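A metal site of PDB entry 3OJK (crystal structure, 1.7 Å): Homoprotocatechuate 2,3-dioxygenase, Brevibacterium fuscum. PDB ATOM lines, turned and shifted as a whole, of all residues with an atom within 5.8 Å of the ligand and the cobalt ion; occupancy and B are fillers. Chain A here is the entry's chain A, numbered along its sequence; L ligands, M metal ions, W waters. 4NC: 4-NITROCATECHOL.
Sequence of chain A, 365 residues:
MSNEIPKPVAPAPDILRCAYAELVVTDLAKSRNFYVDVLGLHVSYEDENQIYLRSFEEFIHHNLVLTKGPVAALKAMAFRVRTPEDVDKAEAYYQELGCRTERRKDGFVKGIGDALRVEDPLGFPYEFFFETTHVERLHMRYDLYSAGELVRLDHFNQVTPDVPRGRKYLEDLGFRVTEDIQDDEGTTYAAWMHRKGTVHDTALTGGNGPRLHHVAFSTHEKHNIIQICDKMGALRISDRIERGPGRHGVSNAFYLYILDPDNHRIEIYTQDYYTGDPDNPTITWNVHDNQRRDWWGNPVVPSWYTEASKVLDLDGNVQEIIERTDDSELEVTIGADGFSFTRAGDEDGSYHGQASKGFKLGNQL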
ATOM      1  N   HIS A 155      11.108  23.973 -25.838  1.00  0.00           N
ATOM      2  CA  HIS A 155      11.615  23.621 -24.487  1.00  0.00           C
ATOM      3  C   HIS A 155      11.859  22.125 -24.290  1.00  0.00           C
ATOM      4  O   HIS A 155      11.430  21.307 -25.090  1.00  0.00           O
ATOM      5  CB  HIS A 155      10.662  24.124 -23.414  1.00  0.00           C
ATOM      6  CG  HIS A 155       9.305  23.484 -23.430  1.00  0.00           C
ATOM      7  ND1 HIS A 155       8.243  24.024 -24.120  1.00  0.00           N
ATOM      8  CD2 HIS A 155       8.839  22.358 -22.840  1.00  0.00           C
ATOM      9  CE1 HIS A 155       7.164  23.265 -23.927  1.00  0.00           C
ATOM     10  NE2 HIS A 155       7.491  22.255 -23.136  1.00  0.00           N
ATOM     11  N   PHE A 156      12.553  21.800 -23.204  1.00  0.00           N
ATOM     12  CA  PHE A 156      12.626  20.470 -22.661  1.00  0.00           C
ATOM     13  C   PHE A 156      11.849  20.421 -21.339  1.00  0.00           C
ATOM     14  O   PHE A 156      11.535  21.472 -20.739  1.00  0.00           O
ATOM     15  CB  PHE A 156      14.072  20.135 -22.312  1.00  0.00           C
ATOM     16  CG  PHE A 156      15.069  20.442 -23.406  1.00  0.00           C
ATOM     17  CD1 PHE A 156      14.925  19.900 -24.671  1.00  0.00           C
ATOM     18  CD2 PHE A 156      16.181  21.230 -23.138  1.00  0.00           C
ATOM     19  CE1 PHE A 156      15.881  20.171 -25.659  1.00  0.00           C
ATOM     20  CE2 PHE A 156      17.129  21.495 -24.129  1.00  0.00           C
ATOM     21  CZ  PHE A 156      16.960  20.975 -25.380  1.00  0.00           C
ATOM     22  N   ASN A 157      11.483  19.226 -20.897  1.00  0.00           N
ATOM     23  CA  ASN A 157      10.929  19.077 -19.544  1.00  0.00           C
ATOM     24  C   ASN A 157      11.575  17.840 -18.909  1.00  0.00           C
ATOM     25  O   ASN A 157      11.590  16.757 -19.505  1.00  0.00           O
ATOM     26  CB  ASN A 157       9.408  18.995 -19.617  1.00  0.00           C
ATOM     27  CG  ASN A 157       8.756  18.957 -18.275  1.00  0.00           C
ATOM     28  OD1 ASN A 157       9.016  18.091 -17.472  1.00  0.00           O
ATOM     29  ND2 ASN A 157       7.876  19.916 -18.024  1.00  0.00           N
ATOM     30  N   ILE A 181       3.954  24.940  -9.561  1.00  0.00           N
ATOM     31  CA  ILE A 181       2.841  24.267  -8.905  1.00  0.00           C
ATOM     32  C   ILE A 181       3.258  23.845  -7.496  1.00  0.00           C
ATOM     33  O   ILE A 181       4.288  23.174  -7.314  1.00  0.00           O
ATOM     34  CB  ILE A 181       2.372  23.028  -9.701  1.00  0.00           C
ATOM     35  CG1 ILE A 181       1.896  23.456 -11.090  1.00  0.00           C
ATOM     36  CG2 ILE A 181       1.236  22.295  -8.895  1.00  0.00           C
ATOM     37  CD1 ILE A 181       1.458  22.251 -12.000  1.00  0.00           C
ATOM     38  N   TRP A 192       8.800  25.945 -13.995  1.00  0.00           N
ATOM     39  CA  TRP A 192       9.143  26.290 -15.348  1.00  0.00           C
ATOM     40  C   TRP A 192      10.079  27.471 -15.284  1.00  0.00           C
ATOM     41  O   TRP A 192       9.857  28.385 -14.472  1.00  0.00           O
ATOM     42  CB  TRP A 192       7.855  26.719 -16.074  1.00  0.00           C
ATOM     43  CG  TRP A 192       6.930  25.591 -16.443  1.00  0.00           C
ATOM     44  CD1 TRP A 192       6.751  25.085 -17.705  1.00  0.00           C
ATOM     45  CD2 TRP A 192       6.029  24.865 -15.602  1.00  0.00           C
ATOM     46  NE1 TRP A 192       5.834  24.080 -17.692  1.00  0.00           N
ATOM     47  CE2 TRP A 192       5.372  23.917 -16.422  1.00  0.00           C
ATOM     48  CE3 TRP A 192       5.694  24.926 -14.245  1.00  0.00           C
ATOM     49  CZ2 TRP A 192       4.414  23.025 -15.922  1.00  0.00           C
ATOM     50  CZ3 TRP A 192       4.747  24.024 -13.748  1.00  0.00           C
ATOM     51  CH2 TRP A 192       4.115  23.089 -14.591  1.00  0.00           C
ATOM     52  N   HIS A 200       9.312  29.031 -20.889  1.00  0.00           N
ATOM     53  CA  HIS A 200      10.424  28.204 -20.496  1.00  0.00           C
ATOM     54  C   HIS A 200      11.337  27.740 -21.632  1.00  0.00           C
ATOM     55  O   HIS A 200      10.954  27.697 -22.814  1.00  0.00           O
ATOM     56  CB  HIS A 200       9.966  26.999 -19.654  1.00  0.00           C
ATOM     57  CG  HIS A 200       8.952  26.092 -20.295  1.00  0.00           C
ATOM     58  ND1 HIS A 200       7.829  26.554 -20.942  1.00  0.00           N
ATOM     59  CD2 HIS A 200       8.843  24.749 -20.270  1.00  0.00           C
ATOM     60  CE1 HIS A 200       7.096  25.520 -21.330  1.00  0.00           C
ATOM     61  NE2 HIS A 200       7.690  24.416 -20.929  1.00  0.00           N
ATOM     62  N   HIS A 214       9.665  15.306 -21.785  1.00  0.00           N
ATOM     63  CA  HIS A 214       9.426  15.580 -23.192  1.00  0.00           C
ATOM     64  C   HIS A 214      10.344  16.638 -23.791  1.00  0.00           C
ATOM     65  O   HIS A 214      11.014  17.357 -23.073  1.00  0.00           O
ATOM     66  CB  HIS A 214       7.947  15.963 -23.403  1.00  0.00           C
ATOM     67  CG  HIS A 214       7.491  17.208 -22.693  1.00  0.00           C
ATOM     68  ND1 HIS A 214       6.919  17.186 -21.438  1.00  0.00           N
ATOM     69  CD2 HIS A 214       7.422  18.493 -23.109  1.00  0.00           C
ATOM     70  CE1 HIS A 214       6.547  18.402 -21.097  1.00  0.00           C
ATOM     71  NE2 HIS A 214       6.843  19.219 -22.091  1.00  0.00           N
ATOM     72  N   ALA A 216       9.667  19.763 -26.711  1.00  0.00           N
ATOM     73  CA  ALA A 216       8.498  20.464 -27.233  1.00  0.00           C
ATOM     74  C   ALA A 216       8.873  21.331 -28.422  1.00  0.00           C
ATOM     75  O   ALA A 216       9.891  22.073 -28.368  1.00  0.00           O
ATOM     76  CB  ALA A 216       7.842  21.321 -26.117  1.00  0.00           C
ATOM     77  N   ARG A 243      -2.188  12.678 -24.821  1.00  0.00           N
ATOM     78  CA  ARG A 243      -2.902  13.661 -24.041  1.00  0.00           C
ATOM     79  C   ARG A 243      -3.143  14.895 -24.884  1.00  0.00           C
ATOM     80  O   ARG A 243      -2.241  15.367 -25.579  1.00  0.00           O
ATOM     81  CB  ARG A 243      -2.099  14.019 -22.784  1.00  0.00           C
ATOM     82  CG  ARG A 243      -2.712  15.075 -21.931  1.00  0.00           C
ATOM     83  CD  ARG A 243      -1.956  15.369 -20.625  1.00  0.00           C
ATOM     84  NE  ARG A 243      -2.458  16.650 -20.156  1.00  0.00           N
ATOM     85  CZ  ARG A 243      -1.747  17.630 -19.631  1.00  0.00           C
ATOM     86  NH1 ARG A 243      -0.453  17.492 -19.317  1.00  0.00           N
ATOM     87  NH2 ARG A 243      -2.354  18.776 -19.357  1.00  0.00           N
ATOM     88  N   HIS A 248      -3.163  24.761 -21.882  1.00  0.00           N
ATOM     89  CA  HIS A 248      -2.533  24.644 -20.561  1.00  0.00           C
ATOM     90  C   HIS A 248      -3.052  25.772 -19.650  1.00  0.00           C
ATOM     91  O   HIS A 248      -3.369  26.883 -20.113  1.00  0.00           O
ATOM     92  CB  HIS A 248      -1.027  24.801 -20.681  1.00  0.00           C
ATOM     93  CG  HIS A 248      -0.298  23.581 -21.149  1.00  0.00           C
ATOM     94  ND1 HIS A 248      -0.494  22.321 -20.598  1.00  0.00           N
ATOM     95  CD2 HIS A 248       0.673  23.443 -22.087  1.00  0.00           C
ATOM     96  CE1 HIS A 248       0.312  21.466 -21.201  1.00  0.00           C
ATOM     97  NE2 HIS A 248       1.038  22.127 -22.094  1.00  0.00           N
ATOM     98  N   GLY A 249      -3.133  25.509 -18.353  1.00  0.00           N
ATOM     99  CA  GLY A 249      -3.208  26.595 -17.389  1.00  0.00           C
ATOM    100  C   GLY A 249      -1.875  27.272 -17.261  1.00  0.00           C
ATOM    101  O   GLY A 249      -1.702  28.403 -17.681  1.00  0.00           O
ATOM    102  N   VAL A 250      -0.953  26.568 -16.622  1.00  0.00           N
ATOM    103  CA  VAL A 250       0.421  27.011 -16.589  1.00  0.00           C
ATOM    104  C   VAL A 250       0.908  27.209 -18.026  1.00  0.00           C
ATOM    105  O   VAL A 250       0.740  26.310 -18.860  1.00  0.00           O
ATOM    106  CB  VAL A 250       1.356  25.950 -15.941  1.00  0.00           C
ATOM    107  CG1 VAL A 250       2.817  26.413 -16.152  1.00  0.00           C
ATOM    108  CG2 VAL A 250       1.040  25.724 -14.441  1.00  0.00           C
ATOM    109  N   SER A 251       1.424  28.393 -18.324  1.00  0.00           N
ATOM    110  CA  SER A 251       1.966  28.770 -19.674  1.00  0.00           C
ATOM    111  C   SER A 251       0.940  29.342 -20.622  1.00  0.00           C
ATOM    112  O   SER A 251       1.295  30.065 -21.549  1.00  0.00           O
ATOM    113  CB  SER A 251       2.717  27.664 -20.408  1.00  0.00           C
ATOM    114  OG  SER A 251       1.860  26.785 -21.110  1.00  0.00           O
ATOM    115  N   TYR A 257       0.323  16.209 -26.620  1.00  0.00           N
ATOM    116  CA  TYR A 257       1.399  15.241 -26.337  1.00  0.00           C
ATOM    117  C   TYR A 257       1.206  13.972 -27.147  1.00  0.00           C
ATOM    118  O   TYR A 257       0.137  13.302 -27.071  1.00  0.00           O
ATOM    119  CB  TYR A 257       1.461  14.864 -24.860  1.00  0.00           C
ATOM    120  CG  TYR A 257       1.731  16.013 -23.938  1.00  0.00           C
ATOM    121  CD1 TYR A 257       3.013  16.467 -23.709  1.00  0.00           C
ATOM    122  CD2 TYR A 257       0.688  16.661 -23.302  1.00  0.00           C
ATOM    123  CE1 TYR A 257       3.264  17.540 -22.878  1.00  0.00           C
ATOM    124  CE2 TYR A 257       0.916  17.734 -22.450  1.00  0.00           C
ATOM    125  CZ  TYR A 257       2.201  18.173 -22.265  1.00  0.00           C
ATOM    126  OH  TYR A 257       2.437  19.188 -21.404  1.00  0.00           O
ATOM    127  N   GLU A 267       5.936  17.131 -27.251  1.00  0.00           N
ATOM    128  CA  GLU A 267       4.828  18.094 -27.145  1.00  0.00           C
ATOM    129  C   GLU A 267       4.832  19.011 -28.341  1.00  0.00           C
ATOM    130  O   GLU A 267       5.898  19.426 -28.796  1.00  0.00           O
ATOM    131  CB  GLU A 267       4.955  18.904 -25.854  1.00  0.00           C
ATOM    132  CG  GLU A 267       3.741  19.799 -25.553  1.00  0.00           C
ATOM    133  CD  GLU A 267       3.938  20.674 -24.331  1.00  0.00           C
ATOM    134  OE1 GLU A 267       5.103  20.808 -23.908  1.00  0.00           O
ATOM    135  OE2 GLU A 267       2.944  21.265 -23.820  1.00  0.00           O
ATOM    136  N   TYR A 269       3.253  22.720 -29.145  1.00  0.00           N
ATOM    137  CA  TYR A 269       3.008  23.803 -28.209  1.00  0.00           C
ATOM    138  C   TYR A 269       2.856  25.112 -28.986  1.00  0.00           C
ATOM    139  O   TYR A 269       3.513  25.283 -30.027  1.00  0.00           O
ATOM    140  CB  TYR A 269       4.209  23.790 -27.247  1.00  0.00           C
ATOM    141  CG  TYR A 269       4.298  24.775 -26.143  1.00  0.00           C
ATOM    142  CD1 TYR A 269       3.856  24.463 -24.867  1.00  0.00           C
ATOM    143  CD2 TYR A 269       4.927  26.005 -26.340  1.00  0.00           C
ATOM    144  CE1 TYR A 269       4.012  25.334 -23.809  1.00  0.00           C
ATOM    145  CE2 TYR A 269       5.066  26.909 -25.278  1.00  0.00           C
ATOM    146  CZ  TYR A 269       4.625  26.538 -24.010  1.00  0.00           C
ATOM    147  OH  TYR A 269       4.824  27.385 -22.966  1.00  0.00           O
ATOM    148  N   ARG A 292      -5.161  23.736 -13.767  1.00  0.00           N
ATOM    149  CA  ARG A 292      -3.735  24.105 -13.827  1.00  0.00           C
ATOM    150  C   ARG A 292      -2.947  23.464 -14.987  1.00  0.00           C
ATOM    151  O   ARG A 292      -2.027  24.075 -15.522  1.00  0.00           O
ATOM    152  CB  ARG A 292      -3.003  23.734 -12.528  1.00  0.00           C
ATOM    153  CG  ARG A 292      -2.673  22.257 -12.439  1.00  0.00           C
ATOM    154  CD  ARG A 292      -2.351  21.796 -11.022  1.00  0.00           C
ATOM    155  NE  ARG A 292      -2.065  20.363 -11.125  1.00  0.00           N
ATOM    156  CZ  ARG A 292      -2.990  19.408 -11.269  1.00  0.00           C
ATOM    157  NH1 ARG A 292      -4.289  19.722 -11.250  1.00  0.00           N
ATOM    158  NH2 ARG A 292      -2.647  18.132 -11.414  1.00  0.00           N
ATOM    159  N   ARG A 293      -3.301  22.253 -15.377  1.00  0.00           N
ATOM    160  CA  ARG A 293      -2.572  21.581 -16.432  1.00  0.00           C
ATOM    161  C   ARG A 293      -3.329  21.643 -17.738  1.00  0.00           C
ATOM    162  O   ARG A 293      -2.756  21.977 -18.768  1.00  0.00           O
ATOM    163  CB  ARG A 293      -2.241  20.151 -16.045  1.00  0.00           C
ATOM    164  CG  ARG A 293      -1.173  20.114 -14.920  1.00  0.00           C
ATOM    165  CD  ARG A 293      -0.338  18.869 -15.010  1.00  0.00           C
ATOM    166  NE  ARG A 293       0.780  18.879 -14.038  1.00  0.00           N
ATOM    167  CZ  ARG A 293       2.018  19.309 -14.292  1.00  0.00           C
ATOM    168  NH1 ARG A 293       2.348  19.817 -15.463  1.00  0.00           N
ATOM    169  NH2 ARG A 293       2.947  19.212 -13.344  1.00  0.00           N
ATOM    170  N   ASP A 294      -4.616  21.332 -17.661  1.00  0.00           N
ATOM    171  CA  ASP A 294      -5.551  21.557 -18.735  1.00  0.00           C
ATOM    172  C   ASP A 294      -6.598  22.544 -18.258  1.00  0.00           C
ATOM    173  O   ASP A 294      -7.407  22.233 -17.358  1.00  0.00           O
ATOM    174  CB  ASP A 294      -6.244  20.254 -19.170  1.00  0.00           C
ATOM    175  CG  ASP A 294      -7.043  20.443 -20.453  1.00  0.00           C
ATOM    176  OD1 ASP A 294      -8.271  20.662 -20.359  1.00  0.00           O
ATOM    177  OD2 ASP A 294      -6.408  20.463 -21.515  1.00  0.00           O
ATOM    178  N   TRP A 304       0.927  10.094 -18.210  1.00  0.00           N
ATOM    179  CA  TRP A 304       1.644  11.355 -18.343  1.00  0.00           C
ATOM    180  C   TRP A 304       2.489  11.654 -17.090  1.00  0.00           C
ATOM    181  O   TRP A 304       3.565  12.262 -17.182  1.00  0.00           O
ATOM    182  CB  TRP A 304       0.620  12.488 -18.636  1.00  0.00           C
ATOM    183  CG  TRP A 304       1.241  13.725 -19.127  1.00  0.00           C
ATOM    184  CD1 TRP A 304       1.459  14.063 -20.439  1.00  0.00           C
ATOM    185  CD2 TRP A 304       1.776  14.776 -18.345  1.00  0.00           C
ATOM    186  NE1 TRP A 304       2.077  15.264 -20.511  1.00  0.00           N
ATOM    187  CE2 TRP A 304       2.291  15.743 -19.242  1.00  0.00           C
ATOM    188  CE3 TRP A 304       1.844  15.028 -16.976  1.00  0.00           C
ATOM    189  CZ2 TRP A 304       2.876  16.934 -18.813  1.00  0.00           C
ATOM    190  CZ3 TRP A 304       2.416  16.214 -16.541  1.00  0.00           C
ATOM    191  CH2 TRP A 304       2.944  17.152 -17.472  1.00  0.00           C
HETATM  192  C1  4NC L   1       4.075  22.821 -20.608  1.00  0.00           C
HETATM  193  C2  4NC L   1       3.833  21.434 -20.178  1.00  0.00           C
HETATM  194  C3  4NC L   1       2.889  21.196 -19.191  1.00  0.00           C
HETATM  195  C4  4NC L   1       2.195  22.252 -18.617  1.00  0.00           C
HETATM  196  C5  4NC L   1       2.436  23.569 -19.028  1.00  0.00           C
HETATM  197  C6  4NC L   1       3.377  23.858 -20.019  1.00  0.00           C
HETATM  198  O7  4NC L   1       4.978  23.028 -21.602  1.00  0.00           O
HETATM  199  O8  4NC L   1       4.506  20.454 -20.800  1.00  0.00           O
HETATM  200  N9  4NC L   1       1.278  21.968 -17.661  1.00  0.00           N
HETATM  201  O10 4NC L   1       0.512  20.621 -17.860  1.00  0.00           O
HETATM  202  O11 4NC L   1       0.386  22.988 -17.547  1.00  0.00           O
HETATM  203 CO    CO M   1       6.021  21.167 -22.050  1.00  0.00          CO
HETATM  204  O   HOH W   1       7.140  21.737 -20.051  1.00  0.00           O
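The backbone carbonyl oxygen (O) of Arg 292 lies close to an oxygen (O11) of the ligand, at 3.3 Å. Residues that only touch the ligand: Trp 192 (3.4 Å), Arg 243 (3.6 Å), Val 250 (3.2 Å), Ser 251 (3.5 Å) and Tyr 269 (3.3 Å). Hydrophobic or aromatic side chains within 4 Å of the ligand: His 155, Trp 192, His 200, His 214, His 248, Val 250, Tyr 257 and Tyr 269. The nearest printed residue that does not touch the ligand is Trp 304 (4.3 Å).
Water W1 bridges ND2 of Asn 157 and NE2 of His 200.
Residues that only touch the cobalt ion: His 200 (3.8 Å). Within 4 Å of the cobalt ion: His 155, His 200, His 214 and Glu 267. The nearest printed residue that does not touch the cobalt ion is Tyr 257 (4.1 Å).
The side-chain hydroxyl (OH) of Tyr 257 lies close to an oxygen (O8) of the ligand (2.5 Å). A ring nitrogen (NE2) of His 200 lies close to an oxygen (O7) of the ligand (3.1 Å). NH1 of Arg 293 lies within hydrogen-bond range of O10 of the ligand (3.1 Å). A ring nitrogen (ND1) of His 248 lies within hydrogen-bond range of an oxygen (O11) of the ligand, 3.2 Å away.
OE2 of Glu 267 is in hydrogen-bond range of OH of Tyr 257. OE2 of Glu 267 is in hydrogen-bond range of NE2 of His 248 (2.7 Å). The backbone carbonyl oxygen of His 155 lies within hydrogen-bond range of the backbone NH of Ala 216 (2.8 Å). The side-chain hydroxyl (OH) of Tyr 257 sits close to a ring nitrogen (NE2) of His 248. The backbone NH (N) of Tyr 257 sits at hydrogen-bond distance from the backbone carbonyl oxygen (O) of Arg 243 (2.9 Å). O of Arg 293 lies within hydrogen-bond range of ND1 of His 248 (2.9 Å). The backbone carbonyl oxygen (O) of Arg 293 sits at hydrogen-bond distance from the guanidinium group (NH2) of Arg 243 (3.3 Å). O of Arg 292 sits close to N of Gly 249 (3.4 Å).
The cobalt ion is bound by an oxygen (O8) of the ligand (2.1 Å), the side-chain carboxylate of Glu 267 (2.1 Å), a ring nitrogen (NE2) of His 214 (2.1 Å), a ring nitrogen (NE2) of His 155 (2.1 Å), an oxygen (O7) of the ligand (2.2 Å) and water W1 (2.4 Å). The cobalt ion has six donor atoms within binding distance.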
